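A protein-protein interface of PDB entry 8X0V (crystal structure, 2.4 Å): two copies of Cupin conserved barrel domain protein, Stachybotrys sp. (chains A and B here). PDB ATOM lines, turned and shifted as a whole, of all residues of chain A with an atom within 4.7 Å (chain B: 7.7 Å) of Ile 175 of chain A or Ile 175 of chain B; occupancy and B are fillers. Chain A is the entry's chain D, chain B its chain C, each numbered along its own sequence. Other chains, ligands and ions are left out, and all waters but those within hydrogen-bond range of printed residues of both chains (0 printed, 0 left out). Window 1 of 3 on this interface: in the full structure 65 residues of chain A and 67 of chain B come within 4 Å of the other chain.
The side-chain hydroxyl of Ser 101 of chain B sits at hydrogen-bond distance from the side-chain hydroxyl of Tyr 124 of chain A, 2.9 Å away.
Val 103 of chain A touches Tyr 124 of chain B.
Ile 122 of chain A touches Tyr 70 of chain B (CD1 to CE2, 3.8 Å).
Tyr 70 of chain B touches Tyr 124 of chain A.
Tyr 124 of chain A touches Val 103 of chain B (CD2 to CG2, 3.5 Å).
CD1 of Ile 126 of chain B touches CE of Met 173 of chain A, 3.9 Å away.
Ile 175 of chain A touches Ile 175 of chain B (CD1 to CD1, 3.6 Å).
CD1 of Leu 177 of chain A touches OG of Ser 101 of chain B, at 3.5 Å.
Of the 10 printed residues of chain A, 6 touch a printed residue of chain B.
Of the 21 printed residues of chain B, 6 touch a printed residue of chain A.
Among the printed residues, 8 pairs touch across the chains.
Among the printed residues, no Asp or Glu carboxylate lies within 4 Å of a Lys or Arg side-chain nitrogen of the other chain.
Val 103 of chain A touches Tyr 124 of chain B, and with the chains exchanged Tyr 124 of chain A touches Val 103 of chain B.
Ile 175 of chain B touches its own counterpart, Ile 175 of chain A.
Positions printed for both chains: 102, 103, 122, 123, 124, 173, 174, 175, 176 and 177.
Of the 8 pairs that touch across the chains among the printed residues, 3 have their exchanged pair printed and touching as well.
The backbone carbonyl oxygen (O) of Tyr 124 of chain A lies within hydrogen-bond range of the backbone NH (N) of Ile 175 of chain A (3.0 Å).
The backbone carbonyl oxygen of Tyr 70 of chain B lies within hydrogen-bond range of the backbone NH of Val 103 of chain B, 2.8 Å away.
O of Ile 122 of chain A is in hydrogen-bond range of N of Leu 177 of chain A, 2.9 Å away.
N of Ile 126 of chain B lies within hydrogen-bond range of O of Met 173 of chain B, 3.0 Å away.
The backbone carbonyl oxygen (O) of Tyr 124 of chain B sits at hydrogen-bond distance from the backbone NH (N) of Ile 175 of chain B, at 2.8 Å.
Of the printed residues of chain B, Val 103 of chain A touches Tyr 124.
Of the printed residues of chain B, Tyr 124 of chain A touches Tyr 70, Ser 101 and Val 103.
Ile 175 of chain A touches just one residue of chain B: Ile 175.
Printed residues of chain B within 4 Å of Leu 177 of chain A: Ser 101 (3.5 Å).
Of the printed residues of chain A, Tyr 70 of chain B touches Ile 122 (3.8 Å) and Tyr 124 (3.7 Å).
Of the printed residues of chain A, Tyr 124 of chain B touches Val 103 (3.5 Å).
Ile 175 of chain B touches just one residue of chain A: Ile 175.
The nearest residue of chain B that does not touch Ile 175 of chain A is Tyr 124 of chain B (4.3 Å).
The nearest residue of chain A that does not touch Ile 175 of chain B is Tyr 124 of chain A (4.4 Å).
The nearest printed residue of chain A that does not touch Ser 101 of chain B is Ile 122 of chain A (6.6 Å).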
ATOM      1  N   ILE A 102       9.226 -18.634 -26.726  1.00  0.00           N
ATOM      2  CA  ILE A 102       8.487 -17.949 -25.672  1.00  0.00           C
ATOM      3  C   ILE A 102       7.205 -18.719 -25.398  1.00  0.00           C
ATOM      4  O   ILE A 102       6.411 -18.957 -26.315  1.00  0.00           O
ATOM      5  CB  ILE A 102       8.153 -16.487 -26.035  1.00  0.00           C
ATOM      6  CG1 ILE A 102       9.428 -15.667 -26.232  1.00  0.00           C
ATOM      7  CG2 ILE A 102       7.284 -15.862 -24.955  1.00  0.00           C
ATOM      8  CD1 ILE A 102       9.205 -14.188 -26.206  1.00  0.00           C
ATOM      9  N   VAL A 103       6.998 -19.100 -24.141  1.00  0.00           N
ATOM     10  CA  VAL A 103       5.739 -19.680 -23.693  1.00  0.00           C
ATOM     11  C   VAL A 103       4.936 -18.543 -23.068  1.00  0.00           C
ATOM     12  O   VAL A 103       5.198 -18.126 -21.936  1.00  0.00           O
ATOM     13  CB  VAL A 103       5.959 -20.832 -22.709  1.00  0.00           C
ATOM     14  CG1 VAL A 103       4.635 -21.515 -22.395  1.00  0.00           C
ATOM     15  CG2 VAL A 103       6.960 -21.827 -23.276  1.00  0.00           C
ATOM     16  N   ILE A 122       6.548 -18.453 -35.936  1.00  0.00           N
ATOM     17  CA  ILE A 122       5.604 -19.557 -36.042  1.00  0.00           C
ATOM     18  C   ILE A 122       5.128 -19.891 -34.632  1.00  0.00           C
ATOM     19  O   ILE A 122       5.936 -20.214 -33.750  1.00  0.00           O
ATOM     20  CB  ILE A 122       6.215 -20.774 -36.762  1.00  0.00           C
ATOM     21  CG1 ILE A 122       5.188 -21.903 -36.879  1.00  0.00           C
ATOM     22  CG2 ILE A 122       7.509 -21.242 -36.098  1.00  0.00           C
ATOM     23  CD1 ILE A 122       5.739 -23.173 -37.493  1.00  0.00           C
ATOM     24  N   ASP A 123       3.822 -19.768 -34.409  1.00  0.00           N
ATOM     25  CA  ASP A 123       3.225 -19.958 -33.094  1.00  0.00           C
ATOM     26  C   ASP A 123       2.422 -21.249 -33.072  1.00  0.00           C
ATOM     27  O   ASP A 123       1.643 -21.519 -33.992  1.00  0.00           O
ATOM     28  CB  ASP A 123       2.311 -18.787 -32.719  1.00  0.00           C
ATOM     29  CG  ASP A 123       2.853 -17.446 -33.169  1.00  0.00           C
ATOM     30  OD1 ASP A 123       4.091 -17.267 -33.169  1.00  0.00           O
ATOM     31  OD2 ASP A 123       2.035 -16.567 -33.518  1.00  0.00           O
ATOM     32  N   TYR A 124       2.617 -22.040 -32.020  1.00  0.00           N
ATOM     33  CA  TYR A 124       1.710 -23.126 -31.675  1.00  0.00           C
ATOM     34  C   TYR A 124       0.726 -22.602 -30.635  1.00  0.00           C
ATOM     35  O   TYR A 124       1.136 -22.157 -29.556  1.00  0.00           O
ATOM     36  CB  TYR A 124       2.467 -24.338 -31.131  1.00  0.00           C
ATOM     37  CG  TYR A 124       3.600 -24.810 -32.010  1.00  0.00           C
ATOM     38  CD1 TYR A 124       3.395 -25.076 -33.356  1.00  0.00           C
ATOM     39  CD2 TYR A 124       4.873 -24.993 -31.489  1.00  0.00           C
ATOM     40  CE1 TYR A 124       4.431 -25.512 -34.162  1.00  0.00           C
ATOM     41  CE2 TYR A 124       5.914 -25.427 -32.286  1.00  0.00           C
ATOM     42  CZ  TYR A 124       5.686 -25.685 -33.622  1.00  0.00           C
ATOM     43  OH  TYR A 124       6.721 -26.119 -34.419  1.00  0.00           O
ATOM     44  N   MET A 173      -2.642 -20.307 -24.690  1.00  0.00           N
ATOM     45  CA  MET A 173      -1.204 -20.447 -24.507  1.00  0.00           C
ATOM     46  C   MET A 173      -0.553 -20.559 -25.873  1.00  0.00           C
ATOM     47  O   MET A 173      -1.023 -21.318 -26.728  1.00  0.00           O
ATOM     48  CB  MET A 173      -0.843 -21.666 -23.652  1.00  0.00           C
ATOM     49  CG  MET A 173       0.609 -21.656 -23.187  1.00  0.00           C
ATOM     50  SD  MET A 173       1.088 -23.115 -22.241  1.00  0.00           S
ATOM     51  CE  MET A 173       1.171 -24.352 -23.535  1.00  0.00           C
ATOM     52  N   TRP A 174       0.518 -19.798 -26.076  1.00  0.00           N
ATOM     53  CA  TRP A 174       1.297 -19.839 -27.302  1.00  0.00           C
ATOM     54  C   TRP A 174       2.732 -20.233 -26.993  1.00  0.00           C
ATOM     55  O   TRP A 174       3.295 -19.827 -25.970  1.00  0.00           O
ATOM     56  CB  TRP A 174       1.294 -18.488 -28.020  1.00  0.00           C
ATOM     57  CG  TRP A 174      -0.038 -18.073 -28.546  1.00  0.00           C
ATOM     58  CD1 TRP A 174      -0.589 -18.418 -29.745  1.00  0.00           C
ATOM     59  CD2 TRP A 174      -0.986 -17.220 -27.898  1.00  0.00           C
ATOM     60  NE1 TRP A 174      -1.827 -17.836 -29.882  1.00  0.00           N
ATOM     61  CE2 TRP A 174      -2.093 -17.095 -28.760  1.00  0.00           C
ATOM     62  CE3 TRP A 174      -1.004 -16.553 -26.671  1.00  0.00           C
ATOM     63  CZ2 TRP A 174      -3.206 -16.329 -28.434  1.00  0.00           C
ATOM     64  CZ3 TRP A 174      -2.111 -15.796 -26.349  1.00  0.00           C
ATOM     65  CH2 TRP A 174      -3.195 -15.685 -27.227  1.00  0.00           C
ATOM     66  N   ILE A 175       3.315 -21.029 -27.877  1.00  0.00           N
ATOM     67  CA  ILE A 175       4.757 -21.213 -27.946  1.00  0.00           C
ATOM     68  C   ILE A 175       5.202 -20.571 -29.250  1.00  0.00           C
ATOM     69  O   ILE A 175       4.881 -21.062 -30.339  1.00  0.00           O
ATOM     70  CB  ILE A 175       5.171 -22.690 -27.874  1.00  0.00           C
ATOM     71  CG1 ILE A 175       4.833 -23.283 -26.505  1.00  0.00           C
ATOM     72  CG2 ILE A 175       6.659 -22.828 -28.142  1.00  0.00           C
ATOM     73  CD1 ILE A 175       3.425 -23.838 -26.400  1.00  0.00           C
ATOM     74  N   LEU A 176       5.912 -19.453 -29.142  1.00  0.00           N
ATOM     75  CA  LEU A 176       6.366 -18.697 -30.301  1.00  0.00           C
ATOM     76  C   LEU A 176       7.807 -19.072 -30.611  1.00  0.00           C
ATOM     77  O   LEU A 176       8.672 -19.015 -29.730  1.00  0.00           O
ATOM     78  CB  LEU A 176       6.252 -17.192 -30.057  1.00  0.00           C
ATOM     79  CG  LEU A 176       4.903 -16.661 -29.563  1.00  0.00           C
ATOM     80  CD1 LEU A 176       4.867 -16.586 -28.048  1.00  0.00           C
ATOM     81  CD2 LEU A 176       4.613 -15.302 -30.171  1.00  0.00           C
ATOM     82  N   LEU A 177       8.059 -19.462 -31.855  1.00  0.00           N
ATOM     83  CA  LEU A 177       9.393 -19.822 -32.306  1.00  0.00           C
ATOM     84  C   LEU A 177       9.852 -18.855 -33.387  1.00  0.00           C
ATOM     85  O   LEU A 177       9.040 -18.276 -34.114  1.00  0.00           O
ATOM     86  CB  LEU A 177       9.436 -21.255 -32.845  1.00  0.00           C
ATOM     87  CG  LEU A 177       9.137 -22.371 -31.848  1.00  0.00           C
ATOM     88  CD1 LEU A 177       9.273 -23.731 -32.514  1.00  0.00           C
ATOM     89  CD2 LEU A 177      10.051 -22.267 -30.637  1.00  0.00           C
ATOM     90  N   TYR B  70       2.675 -30.840 -34.917  1.00  0.00           N
ATOM     91  CA  TYR B  70       3.594 -30.180 -35.837  1.00  0.00           C
ATOM     92  C   TYR B  70       5.022 -30.494 -35.419  1.00  0.00           C
ATOM     93  O   TYR B  70       5.271 -31.039 -34.338  1.00  0.00           O
ATOM     94  CB  TYR B  70       3.378 -28.665 -35.888  1.00  0.00           C
ATOM     95  CG  TYR B  70       3.661 -28.079 -37.252  1.00  0.00           C
ATOM     96  CD1 TYR B  70       2.845 -28.376 -38.336  1.00  0.00           C
ATOM     97  CD2 TYR B  70       4.753 -27.247 -37.460  1.00  0.00           C
ATOM     98  CE1 TYR B  70       3.099 -27.852 -39.589  1.00  0.00           C
ATOM     99  CE2 TYR B  70       5.017 -26.717 -38.710  1.00  0.00           C
ATOM    100  CZ  TYR B  70       4.188 -27.024 -39.771  1.00  0.00           C
ATOM    101  OH  TYR B  70       4.446 -26.500 -41.019  1.00  0.00           O
ATOM    102  N   GLY B 100      15.405 -28.070 -33.776  1.00  0.00           N
ATOM    103  CA  GLY B 100      14.013 -27.992 -34.171  1.00  0.00           C
ATOM    104  C   GLY B 100      13.027 -28.132 -33.029  1.00  0.00           C
ATOM    105  O   GLY B 100      13.352 -27.852 -31.872  1.00  0.00           O
ATOM    106  N   SER B 101      11.813 -28.578 -33.348  1.00  0.00           N
ATOM    107  CA  SER B 101      10.733 -28.658 -32.378  1.00  0.00           C
ATOM    108  C   SER B 101       9.789 -29.780 -32.775  1.00  0.00           C
ATOM    109  O   SER B 101       9.707 -30.149 -33.949  1.00  0.00           O
ATOM    110  CB  SER B 101       9.957 -27.343 -32.288  1.00  0.00           C
ATOM    111  OG  SER B 101       9.255 -27.089 -33.496  1.00  0.00           O
ATOM    112  N   ILE B 102       9.093 -30.334 -31.785  1.00  0.00           N
ATOM    113  CA  ILE B 102       8.026 -31.303 -32.017  1.00  0.00           C
ATOM    114  C   ILE B 102       6.890 -31.004 -31.052  1.00  0.00           C
ATOM    115  O   ILE B 102       7.117 -30.845 -29.848  1.00  0.00           O
ATOM    116  CB  ILE B 102       8.493 -32.763 -31.842  1.00  0.00           C
ATOM    117  CG1 ILE B 102       9.729 -33.048 -32.693  1.00  0.00           C
ATOM    118  CG2 ILE B 102       7.364 -33.724 -32.202  1.00  0.00           C
ATOM    119  CD1 ILE B 102      10.046 -34.502 -32.833  1.00  0.00           C
ATOM    120  N   VAL B 103       5.674 -30.922 -31.576  1.00  0.00           N
ATOM    121  CA  VAL B 103       4.469 -30.811 -30.765  1.00  0.00           C
ATOM    122  C   VAL B 103       3.866 -32.210 -30.704  1.00  0.00           C
ATOM    123  O   VAL B 103       3.223 -32.666 -31.654  1.00  0.00           O
ATOM    124  CB  VAL B 103       3.486 -29.788 -31.337  1.00  0.00           C
ATOM    125  CG1 VAL B 103       2.312 -29.586 -30.384  1.00  0.00           C
ATOM    126  CG2 VAL B 103       4.193 -28.470 -31.605  1.00  0.00           C
ATOM    127  N   ARG B 104       4.084 -32.902 -29.590  1.00  0.00           N
ATOM    128  CA  ARG B 104       3.618 -34.271 -29.414  1.00  0.00           C
ATOM    129  C   ARG B 104       2.508 -34.303 -28.371  1.00  0.00           C
ATOM    130  O   ARG B 104       2.726 -33.937 -27.210  1.00  0.00           O
ATOM    131  CB  ARG B 104       4.765 -35.200 -29.011  1.00  0.00           C
ATOM    132  CG  ARG B 104       4.334 -36.647 -28.811  1.00  0.00           C
ATOM    133  CD  ARG B 104       5.524 -37.577 -28.669  1.00  0.00           C
ATOM    134  NE  ARG B 104       6.216 -37.779 -29.938  1.00  0.00           N
ATOM    135  CZ  ARG B 104       7.435 -37.324 -30.203  1.00  0.00           C
ATOM    136  NH1 ARG B 104       8.109 -36.639 -29.287  1.00  0.00           N
ATOM    137  NH2 ARG B 104       7.986 -37.558 -31.385  1.00  0.00           N
ATOM    138  N   MET B 105       1.325 -34.735 -28.790  1.00  0.00           N
ATOM    139  CA  MET B 105       0.169 -34.894 -27.921  1.00  0.00           C
ATOM    140  C   MET B 105      -0.103 -36.382 -27.738  1.00  0.00           C
ATOM    141  O   MET B 105      -0.077 -37.145 -28.709  1.00  0.00           O
ATOM    142  CB  MET B 105      -1.049 -34.187 -28.525  1.00  0.00           C
ATOM    143  CG  MET B 105      -2.366 -34.426 -27.817  1.00  0.00           C
ATOM    144  SD  MET B 105      -3.694 -33.490 -28.610  1.00  0.00           S
ATOM    145  CE  MET B 105      -3.340 -31.832 -28.037  1.00  0.00           C
ATOM    146  N   SER B 121      16.718 -32.834 -24.036  1.00  0.00           N
ATOM    147  CA  SER B 121      15.594 -32.076 -24.561  1.00  0.00           C
ATOM    148  C   SER B 121      15.023 -31.216 -23.448  1.00  0.00           C
ATOM    149  O   SER B 121      14.939 -31.661 -22.300  1.00  0.00           O
ATOM    150  CB  SER B 121      14.514 -33.017 -25.110  1.00  0.00           C
ATOM    151  OG  SER B 121      13.816 -32.415 -26.179  1.00  0.00           O
ATOM    152  N   ILE B 122      14.646 -29.987 -23.783  1.00  0.00           N
ATOM    153  CA  ILE B 122      13.845 -29.151 -22.895  1.00  0.00           C
ATOM    154  C   ILE B 122      12.397 -29.246 -23.361  1.00  0.00           C
ATOM    155  O   ILE B 122      12.095 -29.023 -24.540  1.00  0.00           O
ATOM    156  CB  ILE B 122      14.366 -27.703 -22.850  1.00  0.00           C
ATOM    157  CG1 ILE B 122      13.642 -26.902 -21.765  1.00  0.00           C
ATOM    158  CG2 ILE B 122      14.289 -27.025 -24.207  1.00  0.00           C
ATOM    159  CD1 ILE B 122      14.277 -25.565 -21.472  1.00  0.00           C
ATOM    160  N   ASP B 123      11.508 -29.643 -22.448  1.00  0.00           N
ATOM    161  CA  ASP B 123      10.137 -30.012 -22.781  1.00  0.00           C
ATOM    162  C   ASP B 123       9.172 -29.037 -22.126  1.00  0.00           C
ATOM    163  O   ASP B 123       9.219 -28.838 -20.907  1.00  0.00           O
ATOM    164  CB  ASP B 123       9.818 -31.440 -22.321  1.00  0.00           C
ATOM    165  CG  ASP B 123      10.749 -32.481 -22.920  1.00  0.00           C
ATOM    166  OD1 ASP B 123      11.595 -32.125 -23.766  1.00  0.00           O
ATOM    167  OD2 ASP B 123      10.630 -33.666 -22.536  1.00  0.00           O
ATOM    168  N   TYR B 124       8.302 -28.434 -22.930  1.00  0.00           N
ATOM    169  CA  TYR B 124       7.159 -27.695 -22.416  1.00  0.00           C
ATOM    170  C   TYR B 124       5.967 -28.641 -22.382  1.00  0.00           C
ATOM    171  O   TYR B 124       5.513 -29.108 -23.431  1.00  0.00           O
ATOM    172  CB  TYR B 124       6.851 -26.473 -23.278  1.00  0.00           C
ATOM    173  CG  TYR B 124       8.007 -25.512 -23.400  1.00  0.00           C
ATOM    174  CD1 TYR B 124       8.827 -25.242 -22.309  1.00  0.00           C
ATOM    175  CD2 TYR B 124       8.289 -24.881 -24.606  1.00  0.00           C
ATOM    176  CE1 TYR B 124       9.888 -24.367 -22.413  1.00  0.00           C
ATOM    177  CE2 TYR B 124       9.349 -24.007 -24.720  1.00  0.00           C
ATOM    178  CZ  TYR B 124      10.144 -23.753 -23.621  1.00  0.00           C
ATOM    179  OH  TYR B 124      11.203 -22.880 -23.729  1.00  0.00           O
ATOM    180  N   GLY B 125       5.474 -28.932 -21.188  1.00  0.00           N
ATOM    181  CA  GLY B 125       4.370 -29.866 -21.013  1.00  0.00           C
ATOM    182  C   GLY B 125       3.170 -29.180 -20.392  1.00  0.00           C
ATOM    183  O   GLY B 125       3.311 -28.395 -19.455  1.00  0.00           O
ATOM    184  N   ILE B 126       1.989 -29.482 -20.925  1.00  0.00           N
ATOM    185  CA  ILE B 126       0.738 -28.957 -20.389  1.00  0.00           C
ATOM    186  C   ILE B 126      -0.274 -30.092 -20.317  1.00  0.00           C
ATOM    187  O   ILE B 126      -0.429 -30.860 -21.273  1.00  0.00           O
ATOM    188  CB  ILE B 126       0.196 -27.777 -21.228  1.00  0.00           C
ATOM    189  CG1 ILE B 126      -1.089 -27.224 -20.608  1.00  0.00           C
ATOM    190  CG2 ILE B 126      -0.025 -28.182 -22.681  1.00  0.00           C
ATOM    191  CD1 ILE B 126      -1.453 -25.835 -21.089  1.00  0.00           C
ATOM    192  N   SER B 150       4.726 -27.780 -17.065  1.00  0.00           N
ATOM    193  CA  SER B 150       6.023 -28.247 -16.598  1.00  0.00           C
ATOM    194  C   SER B 150       7.092 -27.889 -17.620  1.00  0.00           C
ATOM    195  O   SER B 150       6.846 -27.934 -18.829  1.00  0.00           O
ATOM    196  CB  SER B 150       6.010 -29.761 -16.368  1.00  0.00           C
ATOM    197  OG  SER B 150       5.714 -30.452 -17.569  1.00  0.00           O
ATOM    198  N   GLN B 152      10.525 -29.364 -18.448  1.00  0.00           N
ATOM    199  CA  GLN B 152      11.455 -30.467 -18.231  1.00  0.00           C
ATOM    200  C   GLN B 152      12.791 -30.120 -18.873  1.00  0.00           C
ATOM    201  O   GLN B 152      12.889 -30.031 -20.100  1.00  0.00           O
ATOM    202  CB  GLN B 152      10.885 -31.756 -18.814  1.00  0.00           C
ATOM    203  CG  GLN B 152      11.619 -33.011 -18.384  1.00  0.00           C
ATOM    204  CD  GLN B 152      10.925 -33.723 -17.242  1.00  0.00           C
ATOM    205  OE1 GLN B 152      11.532 -34.009 -16.208  1.00  0.00           O
ATOM    206  NE2 GLN B 152       9.643 -34.015 -17.423  1.00  0.00           N
ATOM    207  N   MET B 173       0.142 -32.699 -23.741  1.00  0.00           N
ATOM    208  CA  MET B 173       0.808 -32.169 -24.921  1.00  0.00           C
ATOM    209  C   MET B 173       2.185 -31.656 -24.530  1.00  0.00           C
ATOM    210  O   MET B 173       2.339 -30.969 -23.513  1.00  0.00           O
ATOM    211  CB  MET B 173       0.007 -31.049 -25.593  1.00  0.00           C
ATOM    212  CG  MET B 173       0.552 -30.688 -26.966  1.00  0.00           C
ATOM    213  SD  MET B 173      -0.433 -29.468 -27.848  1.00  0.00           S
ATOM    214  CE  MET B 173      -0.100 -27.999 -26.880  1.00  0.00           C
ATOM    215  N   TRP B 174       3.183 -32.004 -25.334  1.00  0.00           N
ATOM    216  CA  TRP B 174       4.550 -31.548 -25.137  1.00  0.00           C
ATOM    217  C   TRP B 174       5.029 -30.799 -26.369  1.00  0.00           C
ATOM    218  O   TRP B 174       4.664 -31.137 -27.499  1.00  0.00           O
ATOM    219  CB  TRP B 174       5.503 -32.714 -24.860  1.00  0.00           C
ATOM    220  CG  TRP B 174       5.294 -33.381 -23.541  1.00  0.00           C
ATOM    221  CD1 TRP B 174       5.766 -32.969 -22.329  1.00  0.00           C
ATOM    222  CD2 TRP B 174       4.574 -34.593 -23.302  1.00  0.00           C
ATOM    223  NE1 TRP B 174       5.376 -33.847 -21.348  1.00  0.00           N
ATOM    224  CE2 TRP B 174       4.644 -34.854 -21.918  1.00  0.00           C
ATOM    225  CE3 TRP B 174       3.872 -35.482 -24.122  1.00  0.00           C
ATOM    226  CZ2 TRP B 174       4.038 -35.963 -21.335  1.00  0.00           C
ATOM    227  CZ3 TRP B 174       3.273 -36.586 -23.542  1.00  0.00           C
ATOM    228  CH2 TRP B 174       3.362 -36.818 -22.161  1.00  0.00           C
ATOM    229  N   ILE B 175       5.846 -29.778 -26.142  1.00  0.00           N
ATOM    230  CA  ILE B 175       6.655 -29.157 -27.181  1.00  0.00           C
ATOM    231  C   ILE B 175       8.109 -29.392 -26.808  1.00  0.00           C
ATOM    232  O   ILE B 175       8.582 -28.888 -25.781  1.00  0.00           O
ATOM    233  CB  ILE B 175       6.351 -27.659 -27.338  1.00  0.00           C
ATOM    234  CG1 ILE B 175       4.921 -27.449 -27.837  1.00  0.00           C
ATOM    235  CG2 ILE B 175       7.340 -27.019 -28.297  1.00  0.00           C
ATOM    236  CD1 ILE B 175       3.887 -27.354 -26.734  1.00  0.00           C
ATOM    237  N   LEU B 176       8.811 -30.172 -27.619  1.00  0.00           N
ATOM    238  CA  LEU B 176      10.184 -30.559 -27.329  1.00  0.00           C
ATOM    239  C   LEU B 176      11.139 -29.696 -28.136  1.00  0.00           C
ATOM    240  O   LEU B 176      10.988 -29.563 -29.353  1.00  0.00           O
ATOM    241  CB  LEU B 176      10.411 -32.041 -27.635  1.00  0.00           C
ATOM    242  CG  LEU B 176       9.591 -33.009 -26.776  1.00  0.00           C
ATOM    243  CD1 LEU B 176       8.289 -33.400 -27.473  1.00  0.00           C
ATOM    244  CD2 LEU B 176      10.410 -34.240 -26.419  1.00  0.00           C
ATOM    245  N   LEU B 177      12.112 -29.102 -27.452  1.00  0.00           N
ATOM    246  CA  LEU B 177      13.121 -28.265 -28.081  1.00  0.00           C
ATOM    247  C   LEU B 177      14.494 -28.888 -27.886  1.00  0.00           C
ATOM    248  O   LEU B 177      14.734 -29.614 -26.916  1.00  0.00           O
ATOM    249  CB  LEU B 177      13.108 -26.843 -27.509  1.00  0.00           C
ATOM    250  CG  LEU B 177      11.867 -25.990 -27.773  1.00  0.00           C
ATOM    251  CD1 LEU B 177      12.124 -24.544 -27.381  1.00  0.00           C
ATOM    252  CD2 LEU B 177      11.456 -26.087 -29.232  1.00  0.00           C
ATOM    253  N   ASP B 178      15.395 -28.596 -28.819  1.00  0.00           N
ATOM    254  CA  ASP B 178      16.748 -29.123 -28.738  1.00  0.00           C
ATOM    255  C   ASP B 178      17.527 -28.393 -27.653  1.00  0.00           C
ATOM    256  O   ASP B 178      17.417 -27.172 -27.497  1.00  0.00           O
ATOM    257  CB  ASP B 178      17.453 -28.975 -30.085  1.00  0.00           C
ATOM    258  CG  ASP B 178      18.736 -29.782 -30.170  1.00  0.00           C
ATOM    259  OD1 ASP B 178      18.907 -30.724 -29.368  1.00  0.00           O
ATOM    260  OD2 ASP B 178      19.576 -29.474 -31.042  1.00  0.00           O
